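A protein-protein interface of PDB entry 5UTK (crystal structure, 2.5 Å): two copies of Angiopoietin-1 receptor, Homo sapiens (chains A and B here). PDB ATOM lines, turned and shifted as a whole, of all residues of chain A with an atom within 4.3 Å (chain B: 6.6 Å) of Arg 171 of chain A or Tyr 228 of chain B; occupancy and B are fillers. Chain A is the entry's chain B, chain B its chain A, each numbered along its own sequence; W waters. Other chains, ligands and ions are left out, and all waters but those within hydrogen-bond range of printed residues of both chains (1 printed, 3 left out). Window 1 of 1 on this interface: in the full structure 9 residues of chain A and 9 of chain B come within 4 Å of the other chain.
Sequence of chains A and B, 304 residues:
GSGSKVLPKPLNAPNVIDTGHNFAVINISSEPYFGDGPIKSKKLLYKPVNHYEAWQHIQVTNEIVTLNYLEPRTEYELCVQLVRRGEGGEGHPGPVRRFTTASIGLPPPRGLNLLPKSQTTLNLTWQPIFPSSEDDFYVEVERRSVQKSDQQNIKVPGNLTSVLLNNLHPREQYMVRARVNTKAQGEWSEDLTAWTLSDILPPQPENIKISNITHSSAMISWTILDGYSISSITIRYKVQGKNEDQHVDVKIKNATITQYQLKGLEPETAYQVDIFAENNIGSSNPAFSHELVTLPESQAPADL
The guanidinium group (NH2) of Arg 171 of chain B sits at hydrogen-bond distance from the backbone carbonyl oxygen (O) of Arg 171 of chain A.
The backbone NH of Arg 171 of chain B lies within hydrogen-bond range of the side-chain hydroxyl of Thr 196 of chain B, at 2.8 Å.
N of Arg 171 of chain B sits at hydrogen-bond distance from O of Leu 197 of chain B (3.5 Å).
NE1 of Trp 195 of chain B lies within hydrogen-bond range of OD1 of Asp 226 of chain B, at 3.2 Å.
OG1 of Thr 196 of chain A sits at hydrogen-bond distance from N of Arg 171 of chain A, at 3.1 Å.
The backbone NH (N) of Arg 171 of chain A sits at hydrogen-bond distance from the backbone carbonyl oxygen (O) of Leu 197 of chain A (3.3 Å).
N of Glu 172 of chain A lies within hydrogen-bond range of OG1 of Thr 196 of chain A, 2.7 Å away.
Arg 171 of chain A touches Tyr 228 of chain B.
CD1 of Ile 200 of chain B touches CG of Glu 172 of chain A, 3.6 Å away.
Trp 195 of chain A touches Leu 225 of chain B (CZ2 to CD1, 3.5 Å).
Tyr 228 of chain B touches Trp 195 of chain A (OH to CH2, 3.2 Å).
OH of Tyr 228 of chain A touches CH2 of Trp 195 of chain B, 3.4 Å away.
Arg 171 of chain A touches just these residues of chain B: Arg 171 (2.5 Å) and Tyr 228 (3.9 Å).
Of chain A, only Arg 171 and Trp 195 come within 4 Å of Tyr 228 of chain B.
Of the printed residues of chain A, Trp 195 of chain B touches Tyr 228 (3.4 Å).
Of the printed residues of chain A, Ile 200 of chain B touches Glu 172 (3.6 Å).
Of the printed residues of chain A, Leu 225 of chain B touches Trp 195.
Printed residues of chain B within 4 Å of Tyr 228 of chain A: Trp 195.
Pro 202 of chain B touches none of the printed residues of chain A.
The nearest printed residue of chain A that does not touch Tyr 228 of chain B is Gly 227 of chain A (5.0 Å).
The nearest printed residue of chain B that does not touch Trp 195 of chain A is Pro 203 of chain B (4.1 Å).
Hydrophobic or aromatic side chains of chain A within 4 Å of the printed part of chain B: Trp 195 and Tyr 228.
Among the printed residues, 6 pairs touch across the chains.
Among the printed residues, no Asp or Glu carboxylate lies within 4 Å of a Lys or Arg side-chain nitrogen of the other chain.
Arg 171 of chain B touches its own counterpart, Arg 171 of chain A.
Arg 171 of chain A touches Tyr 228 of chain B, but with the chains exchanged Tyr 228 of chain A does not touch Arg 171 of chain B (5.2 Å).
Glu 172 of chain A touches Ile 200 of chain B, but with the chains exchanged Ile 200 of chain A does not touch Glu 172 of chain B (4.3 Å).
Trp 195 of chain A touches Tyr 228 of chain B, and with the chains exchanged Tyr 228 of chain A touches Trp 195 of chain B.
Positions printed for both chains: 170, 171, 172, 195, 196, 197, 198, 200, 227 and 228.
Of the 6 pairs that touch across the chains among the printed residues, 3 have their exchanged pair printed and touching as well.
Water W1 lies within hydrogen-bond range of the side-chain carboxylate (OD2) of Asp 199 of chain A, the guanidinium group (NH1) of Arg 171 of chain A and the side-chain carboxylate (OE2) of Glu 172 of chain B.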
ATOM      1  N   HIS A 169       3.687 -24.369  18.990  1.00  0.00           N
ATOM      2  CA  HIS A 169       2.501 -24.658  18.188  1.00  0.00           C
ATOM      3  C   HIS A 169       2.881 -25.252  16.833  1.00  0.00           C
ATOM      4  O   HIS A 169       3.905 -24.884  16.258  1.00  0.00           O
ATOM      5  CB  HIS A 169       1.653 -23.393  18.011  1.00  0.00           C
ATOM      6  CG  HIS A 169       1.251 -22.753  19.305  1.00  0.00           C
ATOM      7  ND1 HIS A 169       1.575 -21.451  19.623  1.00  0.00           N
ATOM      8  CD2 HIS A 169       0.561 -23.238  20.365  1.00  0.00           C
ATOM      9  CE1 HIS A 169       1.100 -21.162  20.823  1.00  0.00           C
ATOM     10  NE2 HIS A 169       0.480 -22.229  21.294  1.00  0.00           N
ATOM     11  N   PRO A 170       2.059 -26.189  16.329  1.00  0.00           N
ATOM     12  CA  PRO A 170       2.300 -26.854  15.040  1.00  0.00           C
ATOM     13  C   PRO A 170       2.427 -25.863  13.886  1.00  0.00           C
ATOM     14  O   PRO A 170       1.797 -24.803  13.924  1.00  0.00           O
ATOM     15  CB  PRO A 170       1.046 -27.713  14.850  1.00  0.00           C
ATOM     16  CG  PRO A 170       0.536 -27.954  16.231  1.00  0.00           C
ATOM     17  CD  PRO A 170       0.858 -26.710  17.007  1.00  0.00           C
ATOM     18  N   ARG A 171       3.233 -26.207  12.883  1.00  0.00           N
ATOM     19  CA  ARG A 171       3.409 -25.376  11.690  1.00  0.00           C
ATOM     20  C   ARG A 171       3.867 -23.943  11.965  1.00  0.00           C
ATOM     21  O   ARG A 171       3.551 -23.034  11.199  1.00  0.00           O
ATOM     22  CB  ARG A 171       2.132 -25.356  10.837  1.00  0.00           C
ATOM     23  CG  ARG A 171       2.088 -26.413   9.745  1.00  0.00           C
ATOM     24  CD  ARG A 171       0.692 -26.547   9.138  1.00  0.00           C
ATOM     25  NE  ARG A 171       0.257 -25.337   8.446  1.00  0.00           N
ATOM     26  CZ  ARG A 171      -0.881 -24.701   8.697  1.00  0.00           C
ATOM     27  NH1 ARG A 171      -1.711 -25.158   9.624  1.00  0.00           N
ATOM     28  NH2 ARG A 171      -1.193 -23.608   8.017  1.00  0.00           N
ATOM     29  N   GLU A 172       4.609 -23.736  13.048  1.00  0.00           N
ATOM     30  CA  GLU A 172       5.151 -22.407  13.329  1.00  0.00           C
ATOM     31  C   GLU A 172       6.654 -22.320  13.089  1.00  0.00           C
ATOM     32  O   GLU A 172       7.376 -23.310  13.197  1.00  0.00           O
ATOM     33  CB  GLU A 172       4.830 -21.956  14.754  1.00  0.00           C
ATOM     34  CG  GLU A 172       3.434 -21.423  14.944  1.00  0.00           C
ATOM     35  CD  GLU A 172       3.367 -20.384  16.039  1.00  0.00           C
ATOM     36  OE1 GLU A 172       2.424 -20.450  16.855  1.00  0.00           O
ATOM     37  OE2 GLU A 172       4.253 -19.500  16.080  1.00  0.00           O
ATOM     38  N   TRP A 195      11.247 -24.992  11.955  1.00  0.00           N
ATOM     39  CA  TRP A 195       9.797 -25.122  11.987  1.00  0.00           C
ATOM     40  C   TRP A 195       9.371 -26.278  12.880  1.00  0.00           C
ATOM     41  O   TRP A 195      10.029 -27.319  12.919  1.00  0.00           O
ATOM     42  CB  TRP A 195       9.254 -25.379  10.579  1.00  0.00           C
ATOM     43  CG  TRP A 195       9.340 -24.212   9.645  1.00  0.00           C
ATOM     44  CD1 TRP A 195      10.418 -23.835   8.897  1.00  0.00           C
ATOM     45  CD2 TRP A 195       8.296 -23.282   9.343  1.00  0.00           C
ATOM     46  NE1 TRP A 195      10.110 -22.719   8.154  1.00  0.00           N
ATOM     47  CE2 TRP A 195       8.812 -22.361   8.410  1.00  0.00           C
ATOM     48  CE3 TRP A 195       6.973 -23.138   9.772  1.00  0.00           C
ATOM     49  CZ2 TRP A 195       8.053 -21.308   7.901  1.00  0.00           C
ATOM     50  CZ3 TRP A 195       6.221 -22.095   9.267  1.00  0.00           C
ATOM     51  CH2 TRP A 195       6.764 -21.193   8.342  1.00  0.00           C
ATOM     52  N   THR A 196       8.261 -26.102  13.585  1.00  0.00           N
ATOM     53  CA  THR A 196       7.621 -27.230  14.244  1.00  0.00           C
ATOM     54  C   THR A 196       7.093 -28.165  13.158  1.00  0.00           C
ATOM     55  O   THR A 196       6.949 -27.760  12.004  1.00  0.00           O
ATOM     56  CB  THR A 196       6.470 -26.774  15.150  1.00  0.00           C
ATOM     57  OG1 THR A 196       5.806 -25.655  14.550  1.00  0.00           O
ATOM     58  CG2 THR A 196       7.007 -26.356  16.511  1.00  0.00           C
ATOM     59  N   LEU A 197       6.818 -29.414  13.507  1.00  0.00           N
ATOM     60  CA  LEU A 197       6.286 -30.344  12.518  1.00  0.00           C
ATOM     61  C   LEU A 197       4.858 -29.961  12.133  1.00  0.00           C
ATOM     62  O   LEU A 197       4.137 -29.352  12.922  1.00  0.00           O
ATOM     63  CB  LEU A 197       6.346 -31.785  13.028  1.00  0.00           C
ATOM     64  CG  LEU A 197       7.730 -32.431  13.150  1.00  0.00           C
ATOM     65  CD1 LEU A 197       7.589 -33.856  13.656  1.00  0.00           C
ATOM     66  CD2 LEU A 197       8.482 -32.405  11.823  1.00  0.00           C
ATOM     67  N   SER A 198       4.464 -30.310  10.912  1.00  0.00           N
ATOM     68  CA  SER A 198       3.132 -29.995  10.402  1.00  0.00           C
ATOM     69  C   SER A 198       2.043 -30.816  11.081  1.00  0.00           C
ATOM     70  O   SER A 198       2.280 -31.945  11.505  1.00  0.00           O
ATOM     71  CB  SER A 198       3.076 -30.229   8.893  1.00  0.00           C
ATOM     72  OG  SER A 198       1.772 -29.991   8.394  1.00  0.00           O
ATOM     73  N   ASP A 199       0.846 -30.243  11.177  1.00  0.00           N
ATOM     74  CA  ASP A 199      -0.307 -30.966  11.709  1.00  0.00           C
ATOM     75  C   ASP A 199      -1.194 -31.492  10.583  1.00  0.00           C
ATOM     76  O   ASP A 199      -2.155 -32.219  10.831  1.00  0.00           O
ATOM     77  CB  ASP A 199      -1.120 -30.078  12.658  1.00  0.00           C
ATOM     78  CG  ASP A 199      -1.617 -28.809  11.992  1.00  0.00           C
ATOM     79  OD1 ASP A 199      -1.105 -28.466  10.905  1.00  0.00           O
ATOM     80  OD2 ASP A 199      -2.513 -28.148  12.560  1.00  0.00           O
ATOM     81  N   ILE A 200      -0.860 -31.126   9.349  1.00  0.00           N
ATOM     82  CA  ILE A 200      -1.643 -31.524   8.179  1.00  0.00           C
ATOM     83  C   ILE A 200      -0.765 -32.007   7.024  1.00  0.00           C
ATOM     84  O   ILE A 200       0.452 -31.840   7.041  1.00  0.00           O
ATOM     85  CB  ILE A 200      -2.510 -30.356   7.660  1.00  0.00           C
ATOM     86  CG1 ILE A 200      -1.636 -29.125   7.400  1.00  0.00           C
ATOM     87  CG2 ILE A 200      -3.628 -30.038   8.643  1.00  0.00           C
ATOM     88  CD1 ILE A 200      -2.415 -27.879   7.069  1.00  0.00           C
ATOM     89  N   GLY A 227       7.131 -24.393   5.225  1.00  0.00           N
ATOM     90  CA  GLY A 227       6.266 -24.371   6.391  1.00  0.00           C
ATOM     91  C   GLY A 227       5.558 -25.675   6.719  1.00  0.00           C
ATOM     92  O   GLY A 227       4.937 -25.788   7.777  1.00  0.00           O
ATOM     93  N   TYR A 228       5.648 -26.664   5.832  1.00  0.00           N
ATOM     94  CA  TYR A 228       4.930 -27.923   6.041  1.00  0.00           C
ATOM     95  C   TYR A 228       5.836 -29.123   6.332  1.00  0.00           C
ATOM     96  O   TYR A 228       5.400 -30.270   6.211  1.00  0.00           O
ATOM     97  CB  TYR A 228       4.012 -28.224   4.853  1.00  0.00           C
ATOM     98  CG  TYR A 228       2.988 -27.141   4.605  1.00  0.00           C
ATOM     99  CD1 TYR A 228       3.294 -26.045   3.809  1.00  0.00           C
ATOM    100  CD2 TYR A 228       1.721 -27.205   5.177  1.00  0.00           C
ATOM    101  CE1 TYR A 228       2.370 -25.047   3.583  1.00  0.00           C
ATOM    102  CE2 TYR A 228       0.789 -26.209   4.957  1.00  0.00           C
ATOM    103  CZ  TYR A 228       1.121 -25.133   4.158  1.00  0.00           C
ATOM    104  OH  TYR A 228       0.198 -24.136   3.932  1.00  0.00           O
ATOM    105  N   PRO B 170      -7.644 -22.031  11.838  1.00  0.00           N
ATOM    106  CA  PRO B 170      -6.816 -20.942  11.306  1.00  0.00           C
ATOM    107  C   PRO B 170      -5.782 -21.455  10.309  1.00  0.00           C
ATOM    108  O   PRO B 170      -5.369 -22.615  10.395  1.00  0.00           O
ATOM    109  CB  PRO B 170      -6.107 -20.404  12.552  1.00  0.00           C
ATOM    110  CG  PRO B 170      -6.982 -20.794  13.693  1.00  0.00           C
ATOM    111  CD  PRO B 170      -7.595 -22.102  13.308  1.00  0.00           C
ATOM    112  N   ARG B 171      -5.385 -20.596   9.373  1.00  0.00           N
ATOM    113  CA  ARG B 171      -4.330 -20.907   8.407  1.00  0.00           C
ATOM    114  C   ARG B 171      -4.528 -22.195   7.602  1.00  0.00           C
ATOM    115  O   ARG B 171      -3.553 -22.877   7.275  1.00  0.00           O
ATOM    116  CB  ARG B 171      -2.965 -20.933   9.102  1.00  0.00           C
ATOM    117  CG  ARG B 171      -2.515 -19.575   9.610  1.00  0.00           C
ATOM    118  CD  ARG B 171      -1.440 -19.703  10.668  1.00  0.00           C
ATOM    119  NE  ARG B 171      -0.259 -20.399  10.175  1.00  0.00           N
ATOM    120  CZ  ARG B 171       0.386 -21.335  10.861  1.00  0.00           C
ATOM    121  NH1 ARG B 171      -0.041 -21.684  12.067  1.00  0.00           N
ATOM    122  NH2 ARG B 171       1.454 -21.922  10.341  1.00  0.00           N
ATOM    123  N   GLU B 172      -5.773 -22.528   7.275  1.00  0.00           N
ATOM    124  CA  GLU B 172      -6.026 -23.696   6.428  1.00  0.00           C
ATOM    125  C   GLU B 172      -6.765 -23.322   5.146  1.00  0.00           C
ATOM    126  O   GLU B 172      -7.464 -22.300   5.088  1.00  0.00           O
ATOM    127  CB  GLU B 172      -6.782 -24.801   7.178  1.00  0.00           C
ATOM    128  CG  GLU B 172      -5.932 -25.610   8.169  1.00  0.00           C
ATOM    129  CD  GLU B 172      -6.632 -26.872   8.654  1.00  0.00           C
ATOM    130  OE1 GLU B 172      -7.254 -27.571   7.823  1.00  0.00           O
ATOM    131  OE2 GLU B 172      -6.551 -27.173   9.865  1.00  0.00           O
ATOM    132  N   TRP B 195      -8.526 -19.153   2.040  1.00  0.00           N
ATOM    133  CA  TRP B 195      -7.796 -19.414   3.275  1.00  0.00           C
ATOM    134  C   TRP B 195      -8.532 -18.823   4.464  1.00  0.00           C
ATOM    135  O   TRP B 195      -9.047 -17.710   4.390  1.00  0.00           O
ATOM    136  CB  TRP B 195      -6.401 -18.790   3.216  1.00  0.00           C
ATOM    137  CG  TRP B 195      -5.407 -19.538   2.381  1.00  0.00           C
ATOM    138  CD1 TRP B 195      -5.119 -19.330   1.062  1.00  0.00           C
ATOM    139  CD2 TRP B 195      -4.551 -20.601   2.817  1.00  0.00           C
ATOM    140  NE1 TRP B 195      -4.141 -20.208   0.648  1.00  0.00           N
ATOM    141  CE2 TRP B 195      -3.777 -20.999   1.707  1.00  0.00           C
ATOM    142  CE3 TRP B 195      -4.370 -21.262   4.036  1.00  0.00           C
ATOM    143  CZ2 TRP B 195      -2.838 -22.026   1.782  1.00  0.00           C
ATOM    144  CZ3 TRP B 195      -3.438 -22.281   4.108  1.00  0.00           C
ATOM    145  CH2 TRP B 195      -2.684 -22.653   2.988  1.00  0.00           C
ATOM    146  N   THR B 196      -8.576 -19.560   5.566  1.00  0.00           N
ATOM    147  CA  THR B 196      -9.032 -18.990   6.825  1.00  0.00           C
ATOM    148  C   THR B 196      -8.000 -17.965   7.274  1.00  0.00           C
ATOM    149  O   THR B 196      -6.833 -18.051   6.886  1.00  0.00           O
ATOM    150  CB  THR B 196      -9.166 -20.065   7.901  1.00  0.00           C
ATOM    151  OG1 THR B 196      -7.893 -20.697   8.091  1.00  0.00           O
ATOM    152  CG2 THR B 196     -10.175 -21.117   7.472  1.00  0.00           C
ATOM    153  N   LEU B 197      -8.418 -16.992   8.077  1.00  0.00           N
ATOM    154  CA  LEU B 197      -7.492 -15.965   8.549  1.00  0.00           C
ATOM    155  C   LEU B 197      -6.436 -16.532   9.496  1.00  0.00           C
ATOM    156  O   LEU B 197      -6.685 -17.506  10.199  1.00  0.00           O
ATOM    157  CB  LEU B 197      -8.245 -14.822   9.224  1.00  0.00           C
ATOM    158  CG  LEU B 197      -8.977 -13.871   8.281  1.00  0.00           C
ATOM    159  CD1 LEU B 197      -9.531 -12.693   9.058  1.00  0.00           C
ATOM    160  CD2 LEU B 197      -8.050 -13.401   7.172  1.00  0.00           C
ATOM    161  N   SER B 198      -5.260 -15.911   9.512  1.00  0.00           N
ATOM    162  CA  SER B 198      -4.162 -16.361  10.369  1.00  0.00           C
ATOM    163  C   SER B 198      -4.446 -16.130  11.852  1.00  0.00           C
ATOM    164  O   SER B 198      -5.183 -15.215  12.218  1.00  0.00           O
ATOM    165  CB  SER B 198      -2.851 -15.671   9.974  1.00  0.00           C
ATOM    166  OG  SER B 198      -1.763 -16.141  10.758  1.00  0.00           O
ATOM    167  N   ILE B 200      -1.669 -16.087  13.781  1.00  0.00           N
ATOM    168  CA  ILE B 200      -0.353 -15.568  14.141  1.00  0.00           C
ATOM    169  C   ILE B 200       0.190 -14.613  13.082  1.00  0.00           C
ATOM    170  O   ILE B 200      -0.338 -14.527  11.975  1.00  0.00           O
ATOM    171  CB  ILE B 200       0.670 -16.711  14.332  1.00  0.00           C
ATOM    172  CG1 ILE B 200       0.746 -17.575  13.069  1.00  0.00           C
ATOM    173  CG2 ILE B 200       0.311 -17.558  15.547  1.00  0.00           C
ATOM    174  CD1 ILE B 200       1.706 -18.742  13.179  1.00  0.00           C
ATOM    175  N   LEU B 201       1.255 -13.903  13.438  1.00  0.00           N
ATOM    176  CA  LEU B 201       1.919 -12.968  12.537  1.00  0.00           C
ATOM    177  C   LEU B 201       2.589 -13.701  11.381  1.00  0.00           C
ATOM    178  O   LEU B 201       2.984 -14.858  11.526  1.00  0.00           O
ATOM    179  CB  LEU B 201       2.963 -12.164  13.310  1.00  0.00           C
ATOM    180  CG  LEU B 201       2.417 -11.162  14.321  1.00  0.00           C
ATOM    181  CD1 LEU B 201       3.508 -10.766  15.300  1.00  0.00           C
ATOM    182  CD2 LEU B 201       1.873  -9.946  13.597  1.00  0.00           C
ATOM    183  N   PRO B 202       2.725 -13.027  10.229  1.00  0.00           N
ATOM    184  CA  PRO B 202       3.335 -13.671   9.064  1.00  0.00           C
ATOM    185  C   PRO B 202       4.851 -13.788   9.191  1.00  0.00           C
ATOM    186  O   PRO B 202       5.487 -12.898   9.756  1.00  0.00           O
ATOM    187  CB  PRO B 202       2.985 -12.711   7.924  1.00  0.00           C
ATOM    188  CG  PRO B 202       2.905 -11.381   8.578  1.00  0.00           C
ATOM    189  CD  PRO B 202       2.314 -11.641   9.938  1.00  0.00           C
ATOM    190  N   PRO B 203       5.423 -14.894   8.692  1.00  0.00           N
ATOM    191  CA  PRO B 203       6.875 -14.970   8.517  1.00  0.00           C
ATOM    192  C   PRO B 203       7.349 -13.820   7.636  1.00  0.00           C
ATOM    193  O   PRO B 203       6.594 -13.348   6.783  1.00  0.00           O
ATOM    194  CB  PRO B 203       7.066 -16.302   7.786  1.00  0.00           C
ATOM    195  CG  PRO B 203       5.920 -17.140   8.243  1.00  0.00           C
ATOM    196  CD  PRO B 203       4.762 -16.186   8.424  1.00  0.00           C
ATOM    197  N   LEU B 225       5.309 -16.468   2.128  1.00  0.00           N
ATOM    198  CA  LEU B 225       4.667 -17.757   2.342  1.00  0.00           C
ATOM    199  C   LEU B 225       3.158 -17.667   2.169  1.00  0.00           C
ATOM    200  O   LEU B 225       2.500 -16.814   2.770  1.00  0.00           O
ATOM    201  CB  LEU B 225       5.006 -18.301   3.729  1.00  0.00           C
ATOM    202  CG  LEU B 225       6.477 -18.629   3.996  1.00  0.00           C
ATOM    203  CD1 LEU B 225       6.582 -19.546   5.196  1.00  0.00           C
ATOM    204  CD2 LEU B 225       7.136 -19.259   2.776  1.00  0.00           C
ATOM    205  N   ASP B 226       2.618 -18.550   1.335  1.00  0.00           N
ATOM    206  CA  ASP B 226       1.182 -18.635   1.122  1.00  0.00           C
ATOM    207  C   ASP B 226       0.551 -19.229   2.378  1.00  0.00           C
ATOM    208  O   ASP B 226       1.163 -20.066   3.043  1.00  0.00           O
ATOM    209  CB  ASP B 226       0.892 -19.535  -0.080  1.00  0.00           C
ATOM    210  CG  ASP B 226      -0.247 -19.022  -0.939  1.00  0.00           C
ATOM    211  OD1 ASP B 226      -1.398 -18.999  -0.451  1.00  0.00           O
ATOM    212  OD2 ASP B 226       0.007 -18.657  -2.108  1.00  0.00           O
ATOM    213  N   GLY B 227      -0.654 -18.785   2.719  1.00  0.00           N
ATOM    214  CA  GLY B 227      -1.383 -19.377   3.829  1.00  0.00           C
ATOM    215  C   GLY B 227      -1.439 -18.555   5.104  1.00  0.00           C
ATOM    216  O   GLY B 227      -2.001 -19.001   6.106  1.00  0.00           O
ATOM    217  N   TYR B 228      -0.867 -17.354   5.077  1.00  0.00           N
ATOM    218  CA  TYR B 228      -0.872 -16.494   6.255  1.00  0.00           C
ATOM    219  C   TYR B 228      -1.769 -15.264   6.098  1.00  0.00           C
ATOM    220  O   TYR B 228      -1.699 -14.330   6.900  1.00  0.00           O
ATOM    221  CB  TYR B 228       0.554 -16.085   6.632  1.00  0.00           C
ATOM    222  CG  TYR B 228       1.395 -17.259   7.065  1.00  0.00           C
ATOM    223  CD1 TYR B 228       2.111 -18.001   6.135  1.00  0.00           C
ATOM    224  CD2 TYR B 228       1.455 -17.640   8.400  1.00  0.00           C
ATOM    225  CE1 TYR B 228       2.871 -19.081   6.522  1.00  0.00           C
ATOM    226  CE2 TYR B 228       2.216 -18.721   8.797  1.00  0.00           C
ATOM    227  CZ  TYR B 228       2.921 -19.437   7.854  1.00  0.00           C
ATOM    228  OH  TYR B 228       3.676 -20.514   8.243  1.00  0.00           O
ATOM    229  N   SER B 229      -2.615 -15.285   5.070  1.00  0.00           N
ATOM    230  CA  SER B 229      -3.541 -14.188   4.789  1.00  0.00           C
ATOM    231  C   SER B 229      -2.798 -12.861   4.632  1.00  0.00           C
ATOM    232  O   SER B 229      -3.262 -11.813   5.085  1.00  0.00           O
ATOM    233  CB  SER B 229      -4.616 -14.085   5.876  1.00  0.00           C
ATOM    234  OG  SER B 229      -5.105 -15.370   6.228  1.00  0.00           O
ATOM    235  N   ILE B 230      -1.640 -12.918   3.985  1.00  0.00           N
ATOM    236  CA  ILE B 230      -0.854 -11.724   3.721  1.00  0.00           C
ATOM    237  C   ILE B 230      -1.518 -10.860   2.648  1.00  0.00           C
ATOM    238  O   ILE B 230      -1.705 -11.297   1.512  1.00  0.00           O
ATOM    239  CB  ILE B 230       0.592 -12.090   3.327  1.00  0.00           C
ATOM    240  CG1 ILE B 230       1.280 -12.806   4.493  1.00  0.00           C
ATOM    241  CG2 ILE B 230       1.368 -10.847   2.923  1.00  0.00           C
ATOM    242  CD1 ILE B 230       2.698 -13.280   4.200  1.00  0.00           C
ATOM    243  N   SER B 231      -1.871  -9.632   3.023  1.00  0.00           N
ATOM    244  CA  SER B 231      -2.624  -8.735   2.146  1.00  0.00           C
ATOM    245  C   SER B 231      -1.807  -7.551   1.626  1.00  0.00           C
ATOM    246  O   SER B 231      -2.208  -6.894   0.663  1.00  0.00           O
ATOM    247  CB  SER B 231      -3.874  -8.215   2.864  1.00  0.00           C
ATOM    248  OG  SER B 231      -3.537  -7.542   4.068  1.00  0.00           O
ATOM    249  N   GLU B 278       2.338  -7.901   5.699  1.00  0.00           N
ATOM    250  CA  GLU B 278       1.241  -7.580   6.607  1.00  0.00           C
ATOM    251  C   GLU B 278       0.060  -8.533   6.451  1.00  0.00           C
ATOM    252  O   GLU B 278      -0.309  -8.904   5.334  1.00  0.00           O
ATOM    253  CB  GLU B 278       0.766  -6.134   6.404  1.00  0.00           C
ATOM    254  CG  GLU B 278       1.708  -5.072   6.959  1.00  0.00           C
ATOM    255  CD  GLU B 278       2.554  -4.413   5.885  1.00  0.00           C
ATOM    256  OE1 GLU B 278       2.128  -4.412   4.709  1.00  0.00           O
ATOM    257  OE2 GLU B 278       3.642  -3.895   6.221  1.00  0.00           O
ATOM    258  N   ASN B 279      -0.532  -8.925   7.577  1.00  0.00           N
ATOM    259  CA  ASN B 279      -1.791  -9.666   7.556  1.00  0.00           C
ATOM    260  C   ASN B 279      -2.785  -9.191   8.622  1.00  0.00           C
ATOM    261  O   ASN B 279      -2.629  -8.110   9.190  1.00  0.00           O
ATOM    262  CB  ASN B 279      -1.558 -11.177   7.652  1.00  0.00           C
ATOM    263  CG  ASN B 279      -0.975 -11.601   8.983  1.00  0.00           C
ATOM    264  OD1 ASN B 279      -0.712 -10.776   9.855  1.00  0.00           O
ATOM    265  ND2 ASN B 279      -0.776 -12.902   9.148  1.00  0.00           N
ATOM    266  N   ASN B 280      -3.800 -10.009   8.886  1.00  0.00           N
ATOM    267  CA  ASN B 280      -4.868  -9.656   9.819  1.00  0.00           C
ATOM    268  C   ASN B 280      -4.399  -9.461  11.258  1.00  0.00           C
ATOM    269  O   ASN B 280      -4.979  -8.672  12.004  1.00  0.00           O
ATOM    270  CB  ASN B 280      -5.969 -10.716   9.778  1.00  0.00           C
ATOM    271  CG  ASN B 280      -5.431 -12.115   9.990  1.00  0.00           C
ATOM    272  OD1 ASN B 280      -4.674 -12.627   9.166  1.00  0.00           O
ATOM    273  ND2 ASN B 280      -5.825 -12.745  11.091  1.00  0.00           N
ATOM    274  N   ILE B 281      -3.360 -10.191  11.650  1.00  0.00           N
ATOM    275  CA  ILE B 281      -2.798 -10.060  12.989  1.00  0.00           C
ATOM    276  C   ILE B 281      -1.862  -8.854  13.064  1.00  0.00           C
ATOM    277  O   ILE B 281      -1.808  -8.160  14.083  1.00  0.00           O
ATOM    278  CB  ILE B 281      -2.024 -11.330  13.410  1.00  0.00           C
ATOM    279  CG1 ILE B 281      -2.896 -12.577  13.234  1.00  0.00           C
ATOM    280  CG2 ILE B 281      -1.543 -11.216  14.855  1.00  0.00           C
ATOM    281  CD1 ILE B 281      -3.961 -12.734  14.299  1.00  0.00           C
HETATM  282  O   HOH W   1      -3.798 -26.234  11.182  1.00  0.00           O
